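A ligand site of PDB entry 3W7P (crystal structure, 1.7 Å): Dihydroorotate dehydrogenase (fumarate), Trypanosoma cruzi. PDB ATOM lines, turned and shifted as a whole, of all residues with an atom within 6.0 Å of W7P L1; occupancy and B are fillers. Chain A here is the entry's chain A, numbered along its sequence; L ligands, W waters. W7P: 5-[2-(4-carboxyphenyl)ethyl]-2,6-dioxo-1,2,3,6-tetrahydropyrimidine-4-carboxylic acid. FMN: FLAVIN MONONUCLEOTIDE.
The side-chain hydroxyl (OG) of Ser 196 is in hydrogen-bond range of an oxygen (OAC) of W7P L1 (2.7 Å). OD1 of Asn 195 is in hydrogen-bond range of NAN of W7P L1. N of Leu 72 is in hydrogen-bond range of OAF of W7P L1 (2.9 Å). The side-chain amide oxygen of Asn 68 sits at hydrogen-bond distance from a nitrogen (NAM) of W7P L1, 2.9 Å away. OAD of W7P L1 lies within hydrogen-bond range of ND2 of Asn 128, 2.9 Å away. The backbone NH (N) of Gly 71 lies within hydrogen-bond range of an oxygen (OAB) of W7P L1 (3.1 Å). An oxygen (OAF) of W7P L1 is in salt-bridge range of the side-chain amino group (NZ) of Lys 44. An oxygen (OAB) of W7P L1 sits at hydrogen-bond distance from the backbone NH of Met 70, 3.1 Å away. An oxygen (OAA) of W7P L1 lies within salt-bridge range of the side-chain amino group (NZ) of Lys 215, 3.6 Å away. An oxygen (O2) of FMN L2 sits at hydrogen-bond distance from the side-chain amide nitrogen (ND2) of Asn 195, 3.5 Å away. O2 of FMN L2 is in hydrogen-bond range of ND2 of Asn 128 (3.3 Å). The side-chain amino group (NZ) of Lys 44 lies within hydrogen-bond range of an oxygen (O4) of FMN L2 (2.7 Å). The backbone NH of Ser 45 sits close to an oxygen (O4) of FMN L2 (3.4 Å). A nitrogen (N3) of FMN L2 sits at hydrogen-bond distance from the side-chain hydroxyl of Ser 45. An oxygen (O2') of FMN L2 is in hydrogen-bond range of the side-chain amino group (NZ) of Lys 165 (2.9 Å).
Water W3 bridges OAA of W7P L1 (2.7 Å) and N of Asn 133 (2.9 Å). Water W2 lies within hydrogen-bond range of OAE of W7P L1 (2.8 Å), OD1 of Asn 54 (3.2 Å) and NH2 of Arg 51 (3.3 Å). Water W1 lies within hydrogen-bond range of an oxygen (OAB) of W7P L1 (2.9 Å) and the side-chain amide oxygen (OD1) of Asn 68 (3.0 Å).
OAD of W7P L1 lies close to N3 of FMN L2.
Asn 54 touches W7P L1 (ND2 to OAE, 3.7 Å). C of Ser 69 touches OAB of W7P L1, at 3.8 Å. Ser 130 touches W7P L1. O of Cys 131 touches CAJ of W7P L1, at 3.7 Å. Pro 132 touches W7P L1 (CG to CAI, 3.6 Å). Hydrophobic or aromatic side chains that line W7P L1: Met 70, Leu 72 and Pro 132. Within 4 Å of W7P L1: Lys 44, Asn 54, Asn 68, Ser 69, Met 70, Gly 71, Leu 72, Asn 128, Ser 130, Cys 131, Pro 132, Asn 195, Ser 196 and Lys 215.
The side-chain hydroxyl (OG) of Ser 196 lies within hydrogen-bond range of the side-chain amide oxygen (OD1) of Asn 195, 3.4 Å away. OD1 of Asn 128 sits at hydrogen-bond distance from ND2 of Asn 195 (3.4 Å). The guanidinium group (NE) of Arg 51 lies close to the backbone carbonyl oxygen (O) of Leu 72. The side-chain amide oxygen (OD1) of Asn 128 lies within hydrogen-bond range of the backbone NH (N) of Ser 130, 2.9 Å away. The backbone NH (N) of Gly 71 sits close to the side-chain amide nitrogen (ND2) of Asn 54. The backbone carbonyl oxygen (O) of Gly 71 sits at hydrogen-bond distance from the guanidinium group (NH2) of Arg 51 (3.0 Å). The backbone carbonyl oxygen (O) of Ser 130 lies within hydrogen-bond range of the side-chain hydroxyl (OG) of Ser 100. The backbone carbonyl oxygen (O) of Cys 131 sits at hydrogen-bond distance from the side-chain amide nitrogen (NE2) of Gln 139, 2.8 Å away.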
ATOM      1  N   LYS A  44      -2.281 -20.677  -8.901  1.00  0.00           N
ATOM      2  CA  LYS A  44      -2.858 -21.622  -7.926  1.00  0.00           C
ATOM      3  C   LYS A  44      -1.758 -22.065  -7.001  1.00  0.00           C
ATOM      4  O   LYS A  44      -0.663 -22.356  -7.437  1.00  0.00           O
ATOM      5  CB  LYS A  44      -3.383 -22.861  -8.664  1.00  0.00           C
ATOM      6  CG  LYS A  44      -3.872 -24.011  -7.786  1.00  0.00           C
ATOM      7  CD  LYS A  44      -5.033 -23.756  -6.849  1.00  0.00           C
ATOM      8  CE  LYS A  44      -5.240 -24.810  -5.800  1.00  0.00           C
ATOM      9  NZ  LYS A  44      -6.328 -24.489  -4.800  1.00  0.00           N
ATOM     10  N   SER A  45      -2.012 -22.171  -5.707  1.00  0.00           N
ATOM     11  CA  SER A  45      -1.001 -22.717  -4.791  1.00  0.00           C
ATOM     12  C   SER A  45      -0.558 -24.084  -5.246  1.00  0.00           C
ATOM     13  O   SER A  45      -1.401 -24.919  -5.532  1.00  0.00           O
ATOM     14  CB  SER A  45      -1.554 -22.805  -3.415  1.00  0.00           C
ATOM     15  OG  SER A  45      -1.730 -21.490  -2.853  1.00  0.00           O
ATOM     16  N   ARG A  51      -1.347 -32.681  -7.991  1.00  0.00           N
ATOM     17  CA  ARG A  51      -2.417 -33.237  -7.121  1.00  0.00           C
ATOM     18  C   ARG A  51      -3.757 -33.119  -7.793  1.00  0.00           C
ATOM     19  O   ARG A  51      -4.075 -32.145  -8.398  1.00  0.00           O
ATOM     20  CB  ARG A  51      -2.567 -32.496  -5.774  1.00  0.00           C
ATOM     21  CG  ARG A  51      -1.420 -32.601  -4.864  1.00  0.00           C
ATOM     22  CD  ARG A  51      -1.541 -31.645  -3.703  1.00  0.00           C
ATOM     23  NE  ARG A  51      -2.753 -31.889  -2.909  1.00  0.00           N
ATOM     24  CZ  ARG A  51      -2.837 -32.636  -1.819  1.00  0.00           C
ATOM     25  NH1 ARG A  51      -1.779 -33.279  -1.327  1.00  0.00           N
ATOM     26  NH2 ARG A  51      -3.934 -32.710  -1.121  1.00  0.00           N
ATOM     27  N   ASN A  54      -9.431 -33.067  -3.844  1.00  0.00           N
ATOM     28  CA  ASN A  54     -10.515 -33.841  -3.222  1.00  0.00           C
ATOM     29  C   ASN A  54     -11.640 -34.171  -4.159  1.00  0.00           C
ATOM     30  O   ASN A  54     -11.769 -33.640  -5.277  1.00  0.00           O
ATOM     31  CB  ASN A  54     -11.071 -32.984  -2.076  1.00  0.00           C
ATOM     32  CG  ASN A  54     -10.134 -32.819  -0.955  1.00  0.00           C
ATOM     33  OD1 ASN A  54      -9.174 -33.615  -0.758  1.00  0.00           O
ATOM     34  ND2 ASN A  54     -10.362 -31.795  -0.183  1.00  0.00           N
ATOM     35  N   ASN A  68     -15.595 -24.082   0.029  1.00  0.00           N
ATOM     36  CA  ASN A  68     -14.674 -24.971  -0.742  1.00  0.00           C
ATOM     37  C   ASN A  68     -13.826 -25.840   0.143  1.00  0.00           C
ATOM     38  O   ASN A  68     -13.323 -25.461   1.193  1.00  0.00           O
ATOM     39  CB  ASN A  68     -13.770 -24.240  -1.733  1.00  0.00           C
ATOM     40  CG  ASN A  68     -12.448 -23.807  -1.187  1.00  0.00           C
ATOM     41  OD1 ASN A  68     -11.490 -24.544  -1.061  1.00  0.00           O
ATOM     42  ND2 ASN A  68     -12.427 -22.543  -0.674  1.00  0.00           N
ATOM     43  N   SER A  69     -13.588 -27.069  -0.366  1.00  0.00           N
ATOM     44  CA  SER A  69     -12.545 -27.912   0.158  1.00  0.00           C
ATOM     45  C   SER A  69     -11.827 -28.555  -1.001  1.00  0.00           C
ATOM     46  O   SER A  69     -11.796 -29.782  -1.152  1.00  0.00           O
ATOM     47  CB  SER A  69     -13.081 -29.002   1.064  1.00  0.00           C
ATOM     48  OG  SER A  69     -12.000 -29.772   1.523  1.00  0.00           O
ATOM     49  N   MET A  70     -11.255 -27.709  -1.844  1.00  0.00           N
ATOM     50  CA  MET A  70     -10.626 -28.169  -3.099  1.00  0.00           C
ATOM     51  C   MET A  70      -9.590 -29.264  -2.907  1.00  0.00           C
ATOM     52  O   MET A  70      -9.593 -30.201  -3.725  1.00  0.00           O
ATOM     53  CB  MET A  70     -10.006 -27.045  -3.869  1.00  0.00           C
ATOM     54  CG  MET A  70     -10.824 -25.829  -4.202  1.00  0.00           C
ATOM     55  SD  MET A  70     -12.342 -26.218  -5.098  1.00  0.00           S
ATOM     56  CE  MET A  70     -11.730 -26.558  -6.674  1.00  0.00           C
ATOM     57  N   GLY A  71      -8.828 -29.205  -1.841  1.00  0.00           N
ATOM     58  CA  GLY A  71      -7.720 -30.105  -1.565  1.00  0.00           C
ATOM     59  C   GLY A  71      -6.463 -29.873  -2.320  1.00  0.00           C
ATOM     60  O   GLY A  71      -5.736 -30.840  -2.634  1.00  0.00           O
ATOM     61  N   LEU A  72      -6.166 -28.627  -2.665  1.00  0.00           N
ATOM     62  CA  LEU A  72      -4.948 -28.268  -3.329  1.00  0.00           C
ATOM     63  C   LEU A  72      -4.712 -28.972  -4.667  1.00  0.00           C
ATOM     64  O   LEU A  72      -3.549 -29.375  -4.955  1.00  0.00           O
ATOM     65  CB  LEU A  72      -3.762 -28.552  -2.415  1.00  0.00           C
ATOM     66  CG  LEU A  72      -2.952 -27.438  -1.871  1.00  0.00           C
ATOM     67  CD1 LEU A  72      -1.840 -27.949  -0.911  1.00  0.00           C
ATOM     68  CD2 LEU A  72      -2.433 -26.401  -2.891  1.00  0.00           C
ATOM     69  N   PRO A  73      -5.721 -29.081  -5.512  1.00  0.00           N
ATOM     70  CA  PRO A  73      -5.529 -29.616  -6.889  1.00  0.00           C
ATOM     71  C   PRO A  73      -4.628 -28.654  -7.636  1.00  0.00           C
ATOM     72  O   PRO A  73      -4.898 -27.446  -7.597  1.00  0.00           O
ATOM     73  CB  PRO A  73      -6.944 -29.602  -7.518  1.00  0.00           C
ATOM     74  CG  PRO A  73      -7.648 -28.492  -6.723  1.00  0.00           C
ATOM     75  CD  PRO A  73      -7.089 -28.528  -5.340  1.00  0.00           C
ATOM     76  N   SER A 100       2.478 -23.786  -1.718  1.00  0.00           N
ATOM     77  CA  SER A 100       1.861 -24.333  -0.551  1.00  0.00           C
ATOM     78  C   SER A 100       2.329 -25.746  -0.316  1.00  0.00           C
ATOM     79  O   SER A 100       1.588 -26.653  -0.352  1.00  0.00           O
ATOM     80  CB  SER A 100       0.318 -24.231  -0.559  1.00  0.00           C
ATOM     81  OG  SER A 100      -0.152 -24.448   0.737  1.00  0.00           O
ATOM     82  N   ASN A 128       1.851 -19.620   0.895  1.00  0.00           N
ATOM     83  CA  ASN A 128       0.528 -19.907   1.495  1.00  0.00           C
ATOM     84  C   ASN A 128       0.708 -20.774   2.726  1.00  0.00           C
ATOM     85  O   ASN A 128       1.078 -21.930   2.616  1.00  0.00           O
ATOM     86  CB  ASN A 128      -0.352 -20.592   0.502  1.00  0.00           C
ATOM     87  CG  ASN A 128      -1.743 -20.978   1.031  1.00  0.00           C
ATOM     88  OD1 ASN A 128      -2.116 -20.602   2.101  1.00  0.00           O
ATOM     89  ND2 ASN A 128      -2.480 -21.715   0.244  1.00  0.00           N
ATOM     90  N   SER A 130      -1.753 -21.959   4.633  1.00  0.00           N
ATOM     91  CA  SER A 130      -2.858 -22.943   4.857  1.00  0.00           C
ATOM     92  C   SER A 130      -2.565 -24.303   4.233  1.00  0.00           C
ATOM     93  O   SER A 130      -1.825 -24.411   3.260  1.00  0.00           O
ATOM     94  CB  SER A 130      -4.171 -22.314   4.368  1.00  0.00           C
ATOM     95  OG  SER A 130      -4.463 -21.128   5.106  1.00  0.00           O
ATOM     96  N   CYS A 131      -3.091 -25.379   4.810  1.00  0.00           N
ATOM     97  CA  CYS A 131      -2.745 -26.726   4.356  1.00  0.00           C
ATOM     98  C   CYS A 131      -3.836 -27.723   4.787  1.00  0.00           C
ATOM     99  O   CYS A 131      -4.704 -27.418   5.653  1.00  0.00           O
ATOM    100  CB  CYS A 131      -1.403 -27.127   4.989  1.00  0.00           C
ATOM    101  SG  CYS A 131      -1.477 -27.166   6.810  1.00  0.00           S
ATOM    102  N   PRO A 132      -3.792 -28.945   4.208  1.00  0.00           N
ATOM    103  CA  PRO A 132      -4.767 -29.918   4.763  1.00  0.00           C
ATOM    104  C   PRO A 132      -4.603 -30.203   6.241  1.00  0.00           C
ATOM    105  O   PRO A 132      -3.477 -30.084   6.786  1.00  0.00           O
ATOM    106  CB  PRO A 132      -4.501 -31.193   3.937  1.00  0.00           C
ATOM    107  CG  PRO A 132      -3.830 -30.731   2.631  1.00  0.00           C
ATOM    108  CD  PRO A 132      -3.051 -29.474   3.029  1.00  0.00           C
ATOM    109  N   ASN A 133      -5.723 -30.589   6.880  1.00  0.00           N
ATOM    110  CA  ASN A 133      -5.696 -30.941   8.296  1.00  0.00           C
ATOM    111  C   ASN A 133      -4.736 -32.092   8.506  1.00  0.00           C
ATOM    112  O   ASN A 133      -4.773 -33.092   7.770  1.00  0.00           O
ATOM    113  CB  ASN A 133      -7.085 -31.447   8.717  1.00  0.00           C
ATOM    114  CG  ASN A 133      -7.188 -31.762  10.169  1.00  0.00           C
ATOM    115  OD1 ASN A 133      -7.597 -32.878  10.616  1.00  0.00           O
ATOM    116  ND2 ASN A 133      -6.859 -30.794  10.932  1.00  0.00           N
ATOM    117  N   GLN A 139      -3.313 -25.747  11.909  1.00  0.00           N
ATOM    118  CA  GLN A 139      -2.779 -25.060  10.776  1.00  0.00           C
ATOM    119  C   GLN A 139      -1.551 -24.257  11.159  1.00  0.00           C
ATOM    120  O   GLN A 139      -1.507 -23.684  12.215  1.00  0.00           O
ATOM    121  CB  GLN A 139      -3.855 -24.079  10.286  1.00  0.00           C
ATOM    122  CG  GLN A 139      -5.077 -24.748   9.792  1.00  0.00           C
ATOM    123  CD  GLN A 139      -4.818 -25.379   8.465  1.00  0.00           C
ATOM    124  OE1 GLN A 139      -4.568 -24.647   7.479  1.00  0.00           O
ATOM    125  NE2 GLN A 139      -4.895 -26.732   8.391  1.00  0.00           N
ATOM    126  N   LYS A 165       0.522 -15.418   2.594  1.00  0.00           N
ATOM    127  CA  LYS A 165      -0.951 -15.501   2.618  1.00  0.00           C
ATOM    128  C   LYS A 165      -1.378 -16.083   3.951  1.00  0.00           C
ATOM    129  O   LYS A 165      -1.050 -17.206   4.295  1.00  0.00           O
ATOM    130  CB  LYS A 165      -1.413 -16.378   1.479  1.00  0.00           C
ATOM    131  CG  LYS A 165      -2.943 -16.527   1.348  1.00  0.00           C
ATOM    132  CD  LYS A 165      -3.664 -15.283   0.879  1.00  0.00           C
ATOM    133  CE  LYS A 165      -5.128 -15.672   0.608  1.00  0.00           C
ATOM    134  NZ  LYS A 165      -5.323 -16.464  -0.616  1.00  0.00           N
ATOM    135  N   ASN A 195      -7.021 -15.539   3.705  1.00  0.00           N
ATOM    136  CA  ASN A 195      -7.555 -16.828   3.166  1.00  0.00           C
ATOM    137  C   ASN A 195      -9.006 -17.030   3.650  1.00  0.00           C
ATOM    138  O   ASN A 195      -9.588 -16.233   4.421  1.00  0.00           O
ATOM    139  CB  ASN A 195      -6.613 -17.972   3.568  1.00  0.00           C
ATOM    140  CG  ASN A 195      -6.516 -19.047   2.496  1.00  0.00           C
ATOM    141  OD1 ASN A 195      -7.521 -19.523   2.012  1.00  0.00           O
ATOM    142  ND2 ASN A 195      -5.291 -19.470   2.184  1.00  0.00           N
ATOM    143  N   SER A 196      -9.618 -18.095   3.220  1.00  0.00           N
ATOM    144  CA  SER A 196     -10.991 -18.370   3.590  1.00  0.00           C
ATOM    145  C   SER A 196     -11.160 -18.520   5.066  1.00  0.00           C
ATOM    146  O   SER A 196     -10.224 -18.912   5.797  1.00  0.00           O
ATOM    147  CB  SER A 196     -11.487 -19.557   2.734  1.00  0.00           C
ATOM    148  OG  SER A 196     -10.671 -20.615   2.801  1.00  0.00           O
ATOM    149  N   LYS A 215     -14.667 -33.814   3.752  1.00  0.00           N
ATOM    150  CA  LYS A 215     -14.638 -33.303   5.099  1.00  0.00           C
ATOM    151  C   LYS A 215     -16.011 -33.242   5.714  1.00  0.00           C
ATOM    152  O   LYS A 215     -16.274 -32.334   6.506  1.00  0.00           O
ATOM    153  CB  LYS A 215     -13.931 -31.984   5.218  1.00  0.00           C
ATOM    154  CG  LYS A 215     -12.468 -32.051   4.852  1.00  0.00           C
ATOM    155  CD  LYS A 215     -11.908 -30.616   4.830  1.00  0.00           C
ATOM    156  CE  LYS A 215     -12.197 -29.774   6.103  1.00  0.00           C
ATOM    157  NZ  LYS A 215     -11.261 -28.627   6.024  1.00  0.00           N
ATOM    158  N   GLY A 220     -13.779 -24.000   3.624  1.00  0.00           N
ATOM    159  CA  GLY A 220     -13.460 -22.609   3.835  1.00  0.00           C
ATOM    160  C   GLY A 220     -14.514 -21.728   3.169  1.00  0.00           C
ATOM    161  O   GLY A 220     -15.006 -21.925   2.047  1.00  0.00           O
HETATM  162  OAB W7P L   1      -8.717 -26.344  -0.773  1.00  0.00           O
HETATM  163  CAP W7P L   1      -7.822 -25.611  -1.265  1.00  0.00           C
HETATM  164  OAF W7P L   1      -7.132 -25.957  -2.233  1.00  0.00           O
HETATM  165  CAT W7P L   1      -7.609 -24.302  -0.667  1.00  0.00           C
HETATM  166  NAM W7P L   1      -8.834 -23.594  -0.443  1.00  0.00           N
HETATM  167  CAU W7P L   1      -8.782 -22.349   0.179  1.00  0.00           C
HETATM  168  OAC W7P L   1      -9.821 -21.720   0.461  1.00  0.00           O
HETATM  169  NAN W7P L   1      -7.567 -21.876   0.606  1.00  0.00           N
HETATM  170  CAV W7P L   1      -6.368 -22.521   0.363  1.00  0.00           C
HETATM  171  OAD W7P L   1      -5.350 -21.943   0.728  1.00  0.00           O
HETATM  172  CAS W7P L   1      -6.395 -23.780  -0.283  1.00  0.00           C
HETATM  173  CAL W7P L   1      -5.079 -24.516  -0.468  1.00  0.00           C
HETATM  174  CAK W7P L   1      -4.581 -24.979   0.969  1.00  0.00           C
HETATM  175  CAQ W7P L   1      -5.456 -25.953   1.564  1.00  0.00           C
HETATM  176  CAG W7P L   1      -5.395 -27.190   1.007  1.00  0.00           C
HETATM  177  CAI W7P L   1      -6.187 -28.214   1.460  1.00  0.00           C
HETATM  178  CAR W7P L   1      -7.087 -28.055   2.414  1.00  0.00           C
HETATM  179  CAO W7P L   1      -7.846 -29.246   2.744  1.00  0.00           C
HETATM  180  OAE W7P L   1      -7.855 -30.367   2.080  1.00  0.00           O
HETATM  181  OAA W7P L   1      -8.583 -29.152   3.687  1.00  0.00           O
HETATM  182  CAJ W7P L   1      -7.223 -26.807   3.081  1.00  0.00           C
HETATM  183  CAH W7P L   1      -6.390 -25.725   2.569  1.00  0.00           C
HETATM  184  N1  FMN L   2      -6.094 -19.442  -1.290  1.00  0.00           N
HETATM  185  C2  FMN L   2      -4.796 -19.723  -1.534  1.00  0.00           C
HETATM  186  O2  FMN L   2      -3.929 -19.047  -0.959  1.00  0.00           O
HETATM  187  N3  FMN L   2      -4.387 -20.758  -2.329  1.00  0.00           N
HETATM  188  C4  FMN L   2      -5.195 -21.469  -3.022  1.00  0.00           C
HETATM  189  O4  FMN L   2      -4.840 -22.401  -3.827  1.00  0.00           O
HETATM  190  C4A FMN L   2      -6.620 -21.234  -2.864  1.00  0.00           C
HETATM  191  N5  FMN L   2      -7.532 -21.931  -3.550  1.00  0.00           N
HETATM  192  C5A FMN L   2      -8.845 -21.505  -3.562  1.00  0.00           C
HETATM  193  C6  FMN L   2      -9.790 -22.132  -4.324  1.00  0.00           C
HETATM  194  C7  FMN L   2     -11.101 -21.756  -4.368  1.00  0.00           C
HETATM  195  C7M FMN L   2     -12.135 -22.392  -5.282  1.00  0.00           C
HETATM  196  C8  FMN L   2     -11.521 -20.704  -3.549  1.00  0.00           C
HETATM  197  C8M FMN L   2     -12.939 -20.259  -3.513  1.00  0.00           C
HETATM  198  C9  FMN L   2     -10.573 -20.056  -2.779  1.00  0.00           C
HETATM  199  C9A FMN L   2      -9.265 -20.418  -2.705  1.00  0.00           C
HETATM  200  N10 FMN L   2      -8.328 -19.791  -1.913  1.00  0.00           N
HETATM  201  C10 FMN L   2      -7.019 -20.102  -2.009  1.00  0.00           C
HETATM  202  C1' FMN L   2      -8.656 -18.658  -1.012  1.00  0.00           C
HETATM  203  C2' FMN L   2      -8.838 -17.389  -1.779  1.00  0.00           C
HETATM  204  O2' FMN L   2      -7.566 -17.020  -2.315  1.00  0.00           O
HETATM  205  C3' FMN L   2      -9.347 -16.286  -0.915  1.00  0.00           C
HETATM  206  O3' FMN L   2      -8.389 -16.117   0.160  1.00  0.00           O
HETATM  207  C4' FMN L   2     -10.740 -16.587  -0.299  1.00  0.00           C
HETATM  208  O4' FMN L   2     -11.636 -17.226  -1.224  1.00  0.00           O
HETATM  209  C5' FMN L   2     -11.401 -15.334   0.304  1.00  0.00           C
HETATM  210  O5' FMN L   2     -11.594 -14.334  -0.726  1.00  0.00           O
HETATM  211  P   FMN L   2     -13.094 -14.129  -1.398  1.00  0.00           P
HETATM  212  O1P FMN L   2     -12.889 -13.140  -2.481  1.00  0.00           O
HETATM  213  O2P FMN L   2     -14.019 -13.651  -0.264  1.00  0.00           O
HETATM  214  O3P FMN L   2     -13.492 -15.484  -2.000  1.00  0.00           O
HETATM  215  O   HOH W   1     -10.307 -25.514   1.532  1.00  0.00           O
HETATM  216  O   HOH W   2      -6.590 -32.504   0.752  1.00  0.00           O
HETATM  217  O   HOH W   3      -8.277 -31.014   5.614  1.00  0.00           O
